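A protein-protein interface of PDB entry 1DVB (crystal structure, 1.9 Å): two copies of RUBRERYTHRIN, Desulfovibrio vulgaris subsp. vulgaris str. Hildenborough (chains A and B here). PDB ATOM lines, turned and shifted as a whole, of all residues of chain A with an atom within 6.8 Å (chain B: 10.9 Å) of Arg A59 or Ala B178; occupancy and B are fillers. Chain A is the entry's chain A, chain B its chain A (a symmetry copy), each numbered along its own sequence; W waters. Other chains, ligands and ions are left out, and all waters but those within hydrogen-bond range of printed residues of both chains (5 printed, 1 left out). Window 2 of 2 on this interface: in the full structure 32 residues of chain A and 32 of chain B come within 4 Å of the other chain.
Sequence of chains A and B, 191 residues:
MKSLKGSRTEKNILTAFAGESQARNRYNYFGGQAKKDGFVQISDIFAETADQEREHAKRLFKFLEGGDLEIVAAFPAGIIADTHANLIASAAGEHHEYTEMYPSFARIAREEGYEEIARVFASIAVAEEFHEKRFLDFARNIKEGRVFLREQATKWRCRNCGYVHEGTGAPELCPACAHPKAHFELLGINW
OE1 of Glu A55 is in hydrogen-bond range of ND2 of Asn B160 (3.5 Å). NE2 of His A56 sits at hydrogen-bond distance from O of Cys B161, 2.8 Å away. The backbone carbonyl oxygen (O) of Pro B175 sits at hydrogen-bond distance from the guanidinium group (NH1) of Arg A59 (2.9 Å). The backbone carbonyl oxygen (O) of Ala B176 sits at hydrogen-bond distance from the guanidinium group (NH1) of Arg A59.
The backbone carbonyl oxygen (O) of Tyr B163 sits at hydrogen-bond distance from the backbone NH (N) of Cys B158 (2.9 Å). The side-chain amide nitrogen of Asn B160 is in hydrogen-bond range of a ring nitrogen (ND1) of His B179 (3.1 Å). The side-chain sulfur (SG) of Cys B174 lies close to the backbone NH (N) of Ala B176 (3.4 Å).
Among the printed residues, merely in contact across the chains: Arg A59 with Cys B177 (3.96 Å), Arg A59 with Ala B178 (3.7 Å), Ser A123 with Tyr B163 (3.5 Å), Ser A123 with Pro B175 (3.6 Å) and Ser A123 with Ala B176 (3.7 Å).
Of the printed residues of chain B, His A56 touches Cys B161 (2.8 Å). No residue of chain B comes within 4 Å of Ala A57. Printed residues of chain B within 4 Å of Arg A59: Pro B175 (2.9 Å), Ala B176 (2.5 Å), Cys B177 (3.96 Å) and Ala B178 (3.7 Å). Lys A62 touches none of the printed residues of chain B. Of the printed residues of chain A, Asn B160 touches Glu A55 (3.5 Å). Of the printed residues of chain A, Ala B178 touches Arg A59 (3.7 Å). The nearest printed residue of chain A that does not touch Ala B178 is Lys A62 (6.2 Å). The nearest printed residue of chain A that does not touch Tyr B163 is Ile A124 (5.2 Å).
Of the 17 printed residues of chain A, 4 touch a printed residue of chain B. Printed residues of chain A that touch a printed residue of chain B: Glu A55, His A56, Arg A59 and Ser A123. Hydrophobic or aromatic side chains of chain A within 4 Å of the printed part of chain B: His A56. Along chain A the printed residues that touch a printed residue of chain B span positions 55 to 123. Printed residues of chain B that touch a printed residue of chain A: Asn B160, Cys B161, Tyr B163, Pro B175, Ala B176, Cys B177 and Ala B178. Hydrophobic or aromatic side chains of chain B that line the printed part of chain A: Tyr B163, Pro B175, Ala B176 and Ala B178. Among the printed residues, no Asp or Glu carboxylate lies within 4 Å of a Lys or Arg side-chain nitrogen of the other chain.
No position is printed for both chains.
Water W3 lies within hydrogen-bond range of the side-chain hydroxyl of Ser A123 (2.5 Å) and the side-chain hydroxyl of Tyr B163 (3.1 Å). Water W2 bridges the side-chain amide oxygen (OD1) of Asn B160 (3.0 Å) and the side-chain carboxylate (OE2) of Glu A55 (3.4 Å).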
ATOM      1  N   ILE A  13     -18.340  23.654 -32.043  1.00  0.00           N
ATOM      2  CA  ILE A  13     -16.942  24.092 -32.137  1.00  0.00           C
ATOM      3  C   ILE A  13     -16.859  25.392 -32.915  1.00  0.00           C
ATOM      4  O   ILE A  13     -16.217  26.367 -32.489  1.00  0.00           O
ATOM      5  CB  ILE A  13     -16.095  22.998 -32.756  1.00  0.00           C
ATOM      6  CG1 ILE A  13     -15.915  21.760 -31.860  1.00  0.00           C
ATOM      7  CG2 ILE A  13     -14.715  23.499 -33.140  1.00  0.00           C
ATOM      8  CD1 ILE A  13     -15.160  20.699 -32.691  1.00  0.00           C
ATOM      9  N   ARG A  54      -6.904  33.397 -27.816  1.00  0.00           N
ATOM     10  CA  ARG A  54      -6.420  33.003 -29.138  1.00  0.00           C
ATOM     11  C   ARG A  54      -6.035  31.553 -29.130  1.00  0.00           C
ATOM     12  O   ARG A  54      -6.140  30.844 -30.117  1.00  0.00           O
ATOM     13  CB  ARG A  54      -5.224  33.886 -29.519  1.00  0.00           C
ATOM     14  CG  ARG A  54      -4.332  33.250 -30.585  1.00  0.00           C
ATOM     15  CD  ARG A  54      -2.994  33.993 -30.655  1.00  0.00           C
ATOM     16  NE  ARG A  54      -2.030  33.415 -29.713  1.00  0.00           N
ATOM     17  CZ  ARG A  54      -1.064  34.069 -29.100  1.00  0.00           C
ATOM     18  NH1 ARG A  54      -0.854  35.352 -29.274  1.00  0.00           N
ATOM     19  NH2 ARG A  54      -0.271  33.416 -28.276  1.00  0.00           N
ATOM     20  N   GLU A  55      -5.569  31.170 -27.904  1.00  0.00           N
ATOM     21  CA  GLU A  55      -5.046  29.791 -27.874  1.00  0.00           C
ATOM     22  C   GLU A  55      -6.145  28.781 -27.588  1.00  0.00           C
ATOM     23  O   GLU A  55      -6.096  27.625 -27.946  1.00  0.00           O
ATOM     24  CB  GLU A  55      -3.894  29.756 -26.858  1.00  0.00           C
ATOM     25  CG  GLU A  55      -2.747  30.719 -27.192  1.00  0.00           C
ATOM     26  CD  GLU A  55      -1.996  30.152 -28.402  1.00  0.00           C
ATOM     27  OE1 GLU A  55      -1.876  28.919 -28.463  1.00  0.00           O
ATOM     28  OE2 GLU A  55      -1.549  30.937 -29.266  1.00  0.00           O
ATOM     29  N   HIS A  56      -7.224  29.158 -26.927  1.00  0.00           N
ATOM     30  CA  HIS A  56      -8.382  28.296 -26.827  1.00  0.00           C
ATOM     31  C   HIS A  56      -8.975  28.142 -28.247  1.00  0.00           C
ATOM     32  O   HIS A  56      -9.326  27.068 -28.682  1.00  0.00           O
ATOM     33  CB  HIS A  56      -9.481  28.854 -25.931  1.00  0.00           C
ATOM     34  CG  HIS A  56      -9.072  29.071 -24.527  1.00  0.00           C
ATOM     35  ND1 HIS A  56      -9.703  29.954 -23.688  1.00  0.00           N
ATOM     36  CD2 HIS A  56      -8.089  28.493 -23.805  1.00  0.00           C
ATOM     37  CE1 HIS A  56      -9.109  29.918 -22.506  1.00  0.00           C
ATOM     38  NE2 HIS A  56      -8.116  29.033 -22.551  1.00  0.00           N
ATOM     39  N   ALA A  57      -9.083  29.275 -28.953  1.00  0.00           N
ATOM     40  CA  ALA A  57      -9.627  29.235 -30.335  1.00  0.00           C
ATOM     41  C   ALA A  57      -8.811  28.323 -31.205  1.00  0.00           C
ATOM     42  O   ALA A  57      -9.249  27.505 -32.028  1.00  0.00           O
ATOM     43  CB  ALA A  57      -9.710  30.680 -30.847  1.00  0.00           C
ATOM     44  N   LYS A  58      -7.489  28.412 -31.056  1.00  0.00           N
ATOM     45  CA  LYS A  58      -6.680  27.546 -31.912  1.00  0.00           C
ATOM     46  C   LYS A  58      -6.858  26.068 -31.640  1.00  0.00           C
ATOM     47  O   LYS A  58      -6.944  25.274 -32.587  1.00  0.00           O
ATOM     48  CB  LYS A  58      -5.220  27.983 -31.708  1.00  0.00           C
ATOM     49  CG  LYS A  58      -4.251  27.424 -32.747  1.00  0.00           C
ATOM     50  CD  LYS A  58      -2.871  27.345 -32.106  1.00  0.00           C
ATOM     51  CE  LYS A  58      -1.782  27.554 -33.136  1.00  0.00           C
ATOM     52  NZ  LYS A  58      -0.533  28.118 -32.553  1.00  0.00           N
ATOM     53  N   ARG A  59      -6.916  25.597 -30.391  1.00  0.00           N
ATOM     54  CA  ARG A  59      -7.158  24.159 -30.190  1.00  0.00           C
ATOM     55  C   ARG A  59      -8.478  23.747 -30.814  1.00  0.00           C
ATOM     56  O   ARG A  59      -8.579  22.700 -31.446  1.00  0.00           O
ATOM     57  CB  ARG A  59      -7.148  23.851 -28.694  1.00  0.00           C
ATOM     58  CG  ARG A  59      -7.391  22.427 -28.269  1.00  0.00           C
ATOM     59  CD  ARG A  59      -6.291  21.486 -28.666  1.00  0.00           C
ATOM     60  NE  ARG A  59      -6.092  20.271 -27.947  1.00  0.00           N
ATOM     61  CZ  ARG A  59      -6.307  19.807 -26.734  1.00  0.00           C
ATOM     62  NH1 ARG A  59      -6.860  20.538 -25.781  1.00  0.00           N
ATOM     63  NH2 ARG A  59      -5.956  18.551 -26.451  1.00  0.00           N
ATOM     64  N   LEU A  60      -9.505  24.586 -30.639  1.00  0.00           N
ATOM     65  CA  LEU A  60     -10.814  24.291 -31.233  1.00  0.00           C
ATOM     66  C   LEU A  60     -10.758  24.224 -32.761  1.00  0.00           C
ATOM     67  O   LEU A  60     -11.086  23.185 -33.365  1.00  0.00           O
ATOM     68  CB  LEU A  60     -11.865  25.321 -30.791  1.00  0.00           C
ATOM     69  CG  LEU A  60     -12.303  25.174 -29.310  1.00  0.00           C
ATOM     70  CD1 LEU A  60     -13.404  26.142 -28.893  1.00  0.00           C
ATOM     71  CD2 LEU A  60     -12.766  23.740 -28.996  1.00  0.00           C
ATOM     72  N   PHE A  61     -10.336  25.330 -33.377  1.00  0.00           N
ATOM     73  CA  PHE A  61     -10.249  25.446 -34.844  1.00  0.00           C
ATOM     74  C   PHE A  61      -9.546  24.248 -35.431  1.00  0.00           C
ATOM     75  O   PHE A  61      -9.869  23.667 -36.468  1.00  0.00           O
ATOM     76  CB  PHE A  61      -9.531  26.738 -35.202  1.00  0.00           C
ATOM     77  CG  PHE A  61      -9.535  27.077 -36.680  1.00  0.00           C
ATOM     78  CD1 PHE A  61     -10.649  27.698 -37.236  1.00  0.00           C
ATOM     79  CD2 PHE A  61      -8.427  26.770 -37.461  1.00  0.00           C
ATOM     80  CE1 PHE A  61     -10.682  28.036 -38.577  1.00  0.00           C
ATOM     81  CE2 PHE A  61      -8.458  27.106 -38.806  1.00  0.00           C
ATOM     82  CZ  PHE A  61      -9.570  27.727 -39.348  1.00  0.00           C
ATOM     83  N   LYS A  62      -8.499  23.808 -34.711  1.00  0.00           N
ATOM     84  CA  LYS A  62      -7.865  22.618 -35.263  1.00  0.00           C
ATOM     85  C   LYS A  62      -8.756  21.390 -35.289  1.00  0.00           C
ATOM     86  O   LYS A  62      -8.367  20.394 -35.933  1.00  0.00           O
ATOM     87  CB  LYS A  62      -6.629  22.301 -34.420  1.00  0.00           C
ATOM     88  CG  LYS A  62      -5.349  22.688 -35.122  1.00  0.00           C
ATOM     89  CD  LYS A  62      -4.491  23.588 -34.255  1.00  0.00           C
ATOM     90  CE  LYS A  62      -3.211  22.873 -33.812  1.00  0.00           C
ATOM     91  NZ  LYS A  62      -3.403  22.440 -32.392  1.00  0.00           N
ATOM     92  N   PHE A  63      -9.935  21.369 -34.626  1.00  0.00           N
ATOM     93  CA  PHE A  63     -10.627  20.081 -34.763  1.00  0.00           C
ATOM     94  C   PHE A  63     -11.390  20.031 -36.090  1.00  0.00           C
ATOM     95  O   PHE A  63     -11.717  18.935 -36.555  1.00  0.00           O
ATOM     96  CB  PHE A  63     -11.604  19.789 -33.613  1.00  0.00           C
ATOM     97  CG  PHE A  63     -10.923  19.308 -32.345  1.00  0.00           C
ATOM     98  CD1 PHE A  63     -10.331  18.049 -32.300  1.00  0.00           C
ATOM     99  CD2 PHE A  63     -10.882  20.127 -31.222  1.00  0.00           C
ATOM    100  CE1 PHE A  63      -9.686  17.599 -31.157  1.00  0.00           C
ATOM    101  CE2 PHE A  63     -10.241  19.670 -30.068  1.00  0.00           C
ATOM    102  CZ  PHE A  63      -9.656  18.415 -30.030  1.00  0.00           C
ATOM    103  N   LEU A  64     -11.673  21.190 -36.665  1.00  0.00           N
ATOM    104  CA  LEU A  64     -12.514  21.259 -37.866  1.00  0.00           C
ATOM    105  C   LEU A  64     -11.870  20.651 -39.084  1.00  0.00           C
ATOM    106  O   LEU A  64     -10.678  20.755 -39.348  1.00  0.00           O
ATOM    107  CB  LEU A  64     -12.898  22.757 -38.049  1.00  0.00           C
ATOM    108  CG  LEU A  64     -13.653  23.065 -36.726  1.00  0.00           C
ATOM    109  CD1 LEU A  64     -14.064  24.487 -36.622  1.00  0.00           C
ATOM    110  CD2 LEU A  64     -14.837  22.119 -36.667  1.00  0.00           C
ATOM    111  N   GLU A 116     -12.869  13.347 -26.235  1.00  0.00           N
ATOM    112  CA  GLU A 116     -11.685  14.189 -26.190  1.00  0.00           C
ATOM    113  C   GLU A 116     -11.945  15.683 -26.349  1.00  0.00           C
ATOM    114  O   GLU A 116     -11.415  16.570 -25.683  1.00  0.00           O
ATOM    115  CB  GLU A 116     -10.738  13.750 -27.322  1.00  0.00           C
ATOM    116  CG  GLU A 116      -9.962  14.932 -27.881  1.00  0.00           C
ATOM    117  CD  GLU A 116      -8.746  15.364 -27.078  1.00  0.00           C
ATOM    118  OE1 GLU A 116      -8.918  16.031 -26.031  1.00  0.00           O
ATOM    119  OE2 GLU A 116      -7.621  15.028 -27.514  1.00  0.00           O
ATOM    120  N   ARG A 119     -13.443  16.758 -23.354  1.00  0.00           N
ATOM    121  CA  ARG A 119     -12.451  17.131 -22.366  1.00  0.00           C
ATOM    122  C   ARG A 119     -12.000  18.577 -22.532  1.00  0.00           C
ATOM    123  O   ARG A 119     -11.922  19.374 -21.588  1.00  0.00           O
ATOM    124  CB  ARG A 119     -11.229  16.241 -22.513  1.00  0.00           C
ATOM    125  CG  ARG A 119     -11.059  15.136 -21.501  1.00  0.00           C
ATOM    126  CD  ARG A 119     -11.440  13.756 -21.990  1.00  0.00           C
ATOM    127  NE  ARG A 119     -10.372  12.865 -22.378  1.00  0.00           N
ATOM    128  CZ  ARG A 119      -9.066  12.971 -22.528  1.00  0.00           C
ATOM    129  NH1 ARG A 119      -8.375  14.088 -22.318  1.00  0.00           N
ATOM    130  NH2 ARG A 119      -8.383  11.887 -22.917  1.00  0.00           N
ATOM    131  N   VAL A 120     -11.710  18.848 -23.817  1.00  0.00           N
ATOM    132  CA  VAL A 120     -11.218  20.167 -24.178  1.00  0.00           C
ATOM    133  C   VAL A 120     -12.206  21.236 -23.813  1.00  0.00           C
ATOM    134  O   VAL A 120     -11.877  22.330 -23.327  1.00  0.00           O
ATOM    135  CB  VAL A 120     -10.930  20.198 -25.688  1.00  0.00           C
ATOM    136  CG1 VAL A 120     -10.542  21.593 -26.086  1.00  0.00           C
ATOM    137  CG2 VAL A 120      -9.837  19.201 -25.987  1.00  0.00           C
ATOM    138  N   SER A 123     -11.971  21.529 -20.136  1.00  0.00           N
ATOM    139  CA  SER A 123     -10.746  22.178 -19.651  1.00  0.00           C
ATOM    140  C   SER A 123     -10.783  23.654 -19.898  1.00  0.00           C
ATOM    141  O   SER A 123     -10.479  24.467 -19.035  1.00  0.00           O
ATOM    142  CB  SER A 123      -9.592  21.492 -20.351  1.00  0.00           C
ATOM    143  OG  SER A 123      -9.731  20.141 -19.920  1.00  0.00           O
ATOM    144  N   ILE A 124     -11.183  24.100 -21.094  1.00  0.00           N
ATOM    145  CA  ILE A 124     -11.349  25.541 -21.287  1.00  0.00           C
ATOM    146  C   ILE A 124     -12.262  26.222 -20.277  1.00  0.00           C
ATOM    147  O   ILE A 124     -12.034  27.366 -19.824  1.00  0.00           O
ATOM    148  CB  ILE A 124     -11.917  25.779 -22.699  1.00  0.00           C
ATOM    149  CG1 ILE A 124     -10.954  25.320 -23.789  1.00  0.00           C
ATOM    150  CG2 ILE A 124     -12.342  27.230 -22.900  1.00  0.00           C
ATOM    151  CD1 ILE A 124     -11.670  25.315 -25.141  1.00  0.00           C
ATOM    152  N   CYS B 158      -1.218  27.255 -16.584  1.00  0.00           N
ATOM    153  CA  CYS B 158      -0.788  27.263 -17.962  1.00  0.00           C
ATOM    154  C   CYS B 158      -0.641  28.721 -18.422  1.00  0.00           C
ATOM    155  O   CYS B 158      -1.589  29.528 -18.431  1.00  0.00           O
ATOM    156  CB  CYS B 158      -1.779  26.547 -18.867  1.00  0.00           C
ATOM    157  SG  CYS B 158      -1.166  26.417 -20.561  1.00  0.00           S
ATOM    158  N   ARG B 159       0.607  29.042 -18.790  1.00  0.00           N
ATOM    159  CA  ARG B 159       0.873  30.401 -19.250  1.00  0.00           C
ATOM    160  C   ARG B 159       0.263  30.577 -20.636  1.00  0.00           C
ATOM    161  O   ARG B 159      -0.116  31.680 -20.996  1.00  0.00           O
ATOM    162  CB  ARG B 159       2.372  30.681 -19.246  1.00  0.00           C
ATOM    163  CG  ARG B 159       2.848  30.638 -17.796  1.00  0.00           C
ATOM    164  CD  ARG B 159       4.178  31.298 -17.533  1.00  0.00           C
ATOM    165  NE  ARG B 159       3.948  32.776 -17.328  1.00  0.00           N
ATOM    166  CZ  ARG B 159       4.613  33.434 -18.272  1.00  0.00           C
ATOM    167  NH1 ARG B 159       5.263  32.587 -19.084  1.00  0.00           N
ATOM    168  NH2 ARG B 159       4.642  34.722 -18.412  1.00  0.00           N
ATOM    169  N   ASN B 160       0.181  29.452 -21.343  1.00  0.00           N
ATOM    170  CA  ASN B 160      -0.288  29.593 -22.716  1.00  0.00           C
ATOM    171  C   ASN B 160      -1.783  29.863 -22.842  1.00  0.00           C
ATOM    172  O   ASN B 160      -2.142  30.712 -23.687  1.00  0.00           O
ATOM    173  CB  ASN B 160       0.098  28.318 -23.481  1.00  0.00           C
ATOM    174  CG  ASN B 160      -0.149  28.503 -24.987  1.00  0.00           C
ATOM    175  OD1 ASN B 160       0.215  29.540 -25.550  1.00  0.00           O
ATOM    176  ND2 ASN B 160      -0.762  27.458 -25.541  1.00  0.00           N
ATOM    177  N   CYS B 161      -2.607  29.175 -22.028  1.00  0.00           N
ATOM    178  CA  CYS B 161      -4.043  29.316 -22.122  1.00  0.00           C
ATOM    179  C   CYS B 161      -4.726  29.580 -20.779  1.00  0.00           C
ATOM    180  O   CYS B 161      -5.953  29.700 -20.925  1.00  0.00           O
ATOM    181  CB  CYS B 161      -4.800  28.085 -22.650  1.00  0.00           C
ATOM    182  SG  CYS B 161      -4.745  26.638 -21.577  1.00  0.00           S
ATOM    183  N   GLY B 162      -4.066  29.658 -19.644  1.00  0.00           N
ATOM    184  CA  GLY B 162      -4.793  30.000 -18.422  1.00  0.00           C
ATOM    185  C   GLY B 162      -5.379  28.822 -17.676  1.00  0.00           C
ATOM    186  O   GLY B 162      -6.039  28.924 -16.628  1.00  0.00           O
ATOM    187  N   TYR B 163      -5.134  27.625 -18.241  1.00  0.00           N
ATOM    188  CA  TYR B 163      -5.724  26.467 -17.622  1.00  0.00           C
ATOM    189  C   TYR B 163      -5.146  26.307 -16.209  1.00  0.00           C
ATOM    190  O   TYR B 163      -3.923  26.462 -16.141  1.00  0.00           O
ATOM    191  CB  TYR B 163      -5.444  25.194 -18.383  1.00  0.00           C
ATOM    192  CG  TYR B 163      -5.998  23.962 -17.676  1.00  0.00           C
ATOM    193  CD1 TYR B 163      -7.367  23.712 -17.594  1.00  0.00           C
ATOM    194  CD2 TYR B 163      -5.137  23.051 -17.096  1.00  0.00           C
ATOM    195  CE1 TYR B 163      -7.891  22.608 -16.961  1.00  0.00           C
ATOM    196  CE2 TYR B 163      -5.644  21.931 -16.455  1.00  0.00           C
ATOM    197  CZ  TYR B 163      -7.001  21.731 -16.399  1.00  0.00           C
ATOM    198  OH  TYR B 163      -7.446  20.617 -15.764  1.00  0.00           O
ATOM    199  N   PRO B 171       0.995  19.232 -15.103  1.00  0.00           N
ATOM    200  CA  PRO B 171       0.706  18.091 -15.984  1.00  0.00           C
ATOM    201  C   PRO B 171       1.742  17.864 -17.056  1.00  0.00           C
ATOM    202  O   PRO B 171       2.493  18.781 -17.395  1.00  0.00           O
ATOM    203  CB  PRO B 171      -0.600  18.538 -16.678  1.00  0.00           C
ATOM    204  CG  PRO B 171      -0.676  20.017 -16.564  1.00  0.00           C
ATOM    205  CD  PRO B 171       0.069  20.364 -15.307  1.00  0.00           C
ATOM    206  N   GLU B 172       1.852  16.698 -17.679  1.00  0.00           N
ATOM    207  CA  GLU B 172       2.832  16.567 -18.760  1.00  0.00           C
ATOM    208  C   GLU B 172       2.497  17.259 -20.085  1.00  0.00           C
ATOM    209  O   GLU B 172       3.369  17.301 -20.969  1.00  0.00           O
ATOM    210  CB  GLU B 172       3.026  15.072 -19.077  1.00  0.00           C
ATOM    211  CG  GLU B 172       4.435  14.735 -19.528  1.00  0.00           C
ATOM    212  CD  GLU B 172       5.408  14.899 -18.370  1.00  0.00           C
ATOM    213  OE1 GLU B 172       6.212  15.851 -18.428  1.00  0.00           O
ATOM    214  OE2 GLU B 172       5.326  14.073 -17.443  1.00  0.00           O
ATOM    215  N   LEU B 173       1.304  17.759 -20.225  1.00  0.00           N
ATOM    216  CA  LEU B 173       0.571  18.287 -21.348  1.00  0.00           C
ATOM    217  C   LEU B 173      -0.621  19.107 -20.908  1.00  0.00           C
ATOM    218  O   LEU B 173      -1.404  18.669 -20.050  1.00  0.00           O
ATOM    219  CB  LEU B 173       0.093  17.094 -22.164  1.00  0.00           C
ATOM    220  CG  LEU B 173       0.118  17.016 -23.673  1.00  0.00           C
ATOM    221  CD1 LEU B 173      -1.248  16.608 -24.231  1.00  0.00           C
ATOM    222  CD2 LEU B 173       0.539  18.346 -24.284  1.00  0.00           C
ATOM    223  N   CYS B 174      -0.824  20.306 -21.440  1.00  0.00           N
ATOM    224  CA  CYS B 174      -2.030  20.975 -20.969  1.00  0.00           C
ATOM    225  C   CYS B 174      -3.285  20.324 -21.577  1.00  0.00           C
ATOM    226  O   CYS B 174      -3.470  20.133 -22.794  1.00  0.00           O
ATOM    227  CB  CYS B 174      -1.941  22.466 -21.292  1.00  0.00           C
ATOM    228  SG  CYS B 174      -3.391  23.380 -20.735  1.00  0.00           S
ATOM    229  N   PRO B 175      -4.232  19.932 -20.704  1.00  0.00           N
ATOM    230  CA  PRO B 175      -5.508  19.375 -21.157  1.00  0.00           C
ATOM    231  C   PRO B 175      -6.288  20.367 -22.027  1.00  0.00           C
ATOM    232  O   PRO B 175      -6.993  19.947 -22.947  1.00  0.00           O
ATOM    233  CB  PRO B 175      -6.296  19.105 -19.874  1.00  0.00           C
ATOM    234  CG  PRO B 175      -5.448  19.503 -18.724  1.00  0.00           C
ATOM    235  CD  PRO B 175      -4.123  19.990 -19.230  1.00  0.00           C
ATOM    236  N   ALA B 176      -6.180  21.666 -21.761  1.00  0.00           N
ATOM    237  CA  ALA B 176      -6.894  22.670 -22.560  1.00  0.00           C
ATOM    238  C   ALA B 176      -6.161  22.994 -23.868  1.00  0.00           C
ATOM    239  O   ALA B 176      -6.814  22.878 -24.907  1.00  0.00           O
ATOM    240  CB  ALA B 176      -7.147  23.953 -21.755  1.00  0.00           C
ATOM    241  N   CYS B 177      -4.886  23.381 -23.861  1.00  0.00           N
ATOM    242  CA  CYS B 177      -4.224  23.835 -25.086  1.00  0.00           C
ATOM    243  C   CYS B 177      -3.238  22.825 -25.607  1.00  0.00           C
ATOM    244  O   CYS B 177      -2.664  23.005 -26.693  1.00  0.00           O
ATOM    245  CB  CYS B 177      -3.556  25.187 -24.784  1.00  0.00           C
ATOM    246  SG  CYS B 177      -2.017  25.024 -23.835  1.00  0.00           S
ATOM    247  N   ALA B 178      -3.014  21.736 -24.877  1.00  0.00           N
ATOM    248  CA  ALA B 178      -2.104  20.689 -25.359  1.00  0.00           C
ATOM    249  C   ALA B 178      -0.657  21.151 -25.535  1.00  0.00           C
ATOM    250  O   ALA B 178       0.165  20.549 -26.242  1.00  0.00           O
ATOM    251  CB  ALA B 178      -2.612  20.094 -26.673  1.00  0.00           C
ATOM    252  N   HIS B 179      -0.281  22.244 -24.876  1.00  0.00           N
ATOM    253  CA  HIS B 179       1.131  22.608 -24.787  1.00  0.00           C
ATOM    254  C   HIS B 179       1.746  21.811 -23.630  1.00  0.00           C
ATOM    255  O   HIS B 179       1.133  21.331 -22.667  1.00  0.00           O
ATOM    256  CB  HIS B 179       1.248  24.119 -24.653  1.00  0.00           C
ATOM    257  CG  HIS B 179       0.998  24.817 -25.952  1.00  0.00           C
ATOM    258  ND1 HIS B 179      -0.129  24.612 -26.718  1.00  0.00           N
ATOM    259  CD2 HIS B 179       1.740  25.730 -26.638  1.00  0.00           C
ATOM    260  CE1 HIS B 179      -0.096  25.352 -27.822  1.00  0.00           C
ATOM    261  NE2 HIS B 179       1.031  26.037 -27.783  1.00  0.00           N
ATOM    262  N   PRO B 180       3.055  21.574 -23.681  1.00  0.00           N
ATOM    263  CA  PRO B 180       3.722  20.781 -22.642  1.00  0.00           C
ATOM    264  C   PRO B 180       3.979  21.524 -21.332  1.00  0.00           C
ATOM    265  O   PRO B 180       3.782  22.724 -21.183  1.00  0.00           O
ATOM    266  CB  PRO B 180       5.087  20.436 -23.277  1.00  0.00           C
ATOM    267  CG  PRO B 180       5.271  21.350 -24.435  1.00  0.00           C
ATOM    268  CD  PRO B 180       3.962  22.023 -24.744  1.00  0.00           C
ATOM    269  N   LYS B 181       4.436  20.717 -20.375  1.00  0.00           N
ATOM    270  CA  LYS B 181       4.619  21.117 -18.988  1.00  0.00           C
ATOM    271  C   LYS B 181       5.391  22.417 -18.843  1.00  0.00           C
ATOM    272  O   LYS B 181       5.187  23.204 -17.919  1.00  0.00           O
ATOM    273  CB  LYS B 181       5.326  19.958 -18.261  1.00  0.00           C
ATOM    274  CG  LYS B 181       5.865  20.405 -16.908  1.00  0.00           C
ATOM    275  CD  LYS B 181       6.093  19.233 -15.959  1.00  0.00           C
ATOM    276  CE  LYS B 181       6.968  18.161 -16.563  1.00  0.00           C
ATOM    277  NZ  LYS B 181       7.397  17.060 -15.638  1.00  0.00           N
ATOM    278  N   ALA B 182       6.288  22.666 -19.799  1.00  0.00           N
ATOM    279  CA  ALA B 182       7.135  23.838 -19.752  1.00  0.00           C
ATOM    280  C   ALA B 182       6.369  25.145 -19.649  1.00  0.00           C
ATOM    281  O   ALA B 182       6.985  26.137 -19.201  1.00  0.00           O
ATOM    282  CB  ALA B 182       8.012  23.908 -20.995  1.00  0.00           C
ATOM    283  N   HIS B 183       5.098  25.133 -20.035  1.00  0.00           N
ATOM    284  CA  HIS B 183       4.283  26.341 -19.997  1.00  0.00           C
ATOM    285  C   HIS B 183       3.669  26.647 -18.638  1.00  0.00           C
ATOM    286  O   HIS B 183       3.114  27.735 -18.419  1.00  0.00           O
ATOM    287  CB  HIS B 183       3.173  26.181 -21.072  1.00  0.00           C
ATOM    288  CG  HIS B 183       3.803  26.301 -22.429  1.00  0.00           C
ATOM    289  ND1 HIS B 183       3.857  27.511 -23.090  1.00  0.00           N
ATOM    290  CD2 HIS B 183       4.401  25.395 -23.236  1.00  0.00           C
ATOM    291  CE1 HIS B 183       4.465  27.334 -24.265  1.00  0.00           C
ATOM    292  NE2 HIS B 183       4.813  26.060 -24.388  1.00  0.00           N
ATOM    293  N   PHE B 184       3.778  25.678 -17.738  1.00  0.00           N
ATOM    294  CA  PHE B 184       3.139  25.851 -16.414  1.00  0.00           C
ATOM    295  C   PHE B 184       3.946  26.598 -15.377  1.00  0.00           C
ATOM    296  O   PHE B 184       5.191  26.536 -15.356  1.00  0.00           O
ATOM    297  CB  PHE B 184       2.792  24.440 -15.863  1.00  0.00           C
ATOM    298  CG  PHE B 184       1.482  23.974 -16.513  1.00  0.00           C
ATOM    299  CD1 PHE B 184       0.263  24.366 -15.950  1.00  0.00           C
ATOM    300  CD2 PHE B 184       1.542  23.171 -17.648  1.00  0.00           C
ATOM    301  CE1 PHE B 184      -0.921  23.958 -16.528  1.00  0.00           C
ATOM    302  CE2 PHE B 184       0.345  22.758 -18.241  1.00  0.00           C
ATOM    303  CZ  PHE B 184      -0.855  23.151 -17.671  1.00  0.00           C
HETATM  304  O   HOH W   1       0.567  27.790 -29.548  1.00  0.00           O
HETATM  305  O   HOH W   2       1.605  30.154 -28.176  1.00  0.00           O
HETATM  306  O   HOH W   3      -9.698  19.364 -17.541  1.00  0.00           O
HETATM  307  O   HOH W   4      -3.250  23.911 -29.639  1.00  0.00           O
HETATM  308  O   HOH W   5      -4.377  18.116 -24.305  1.00  0.00           O
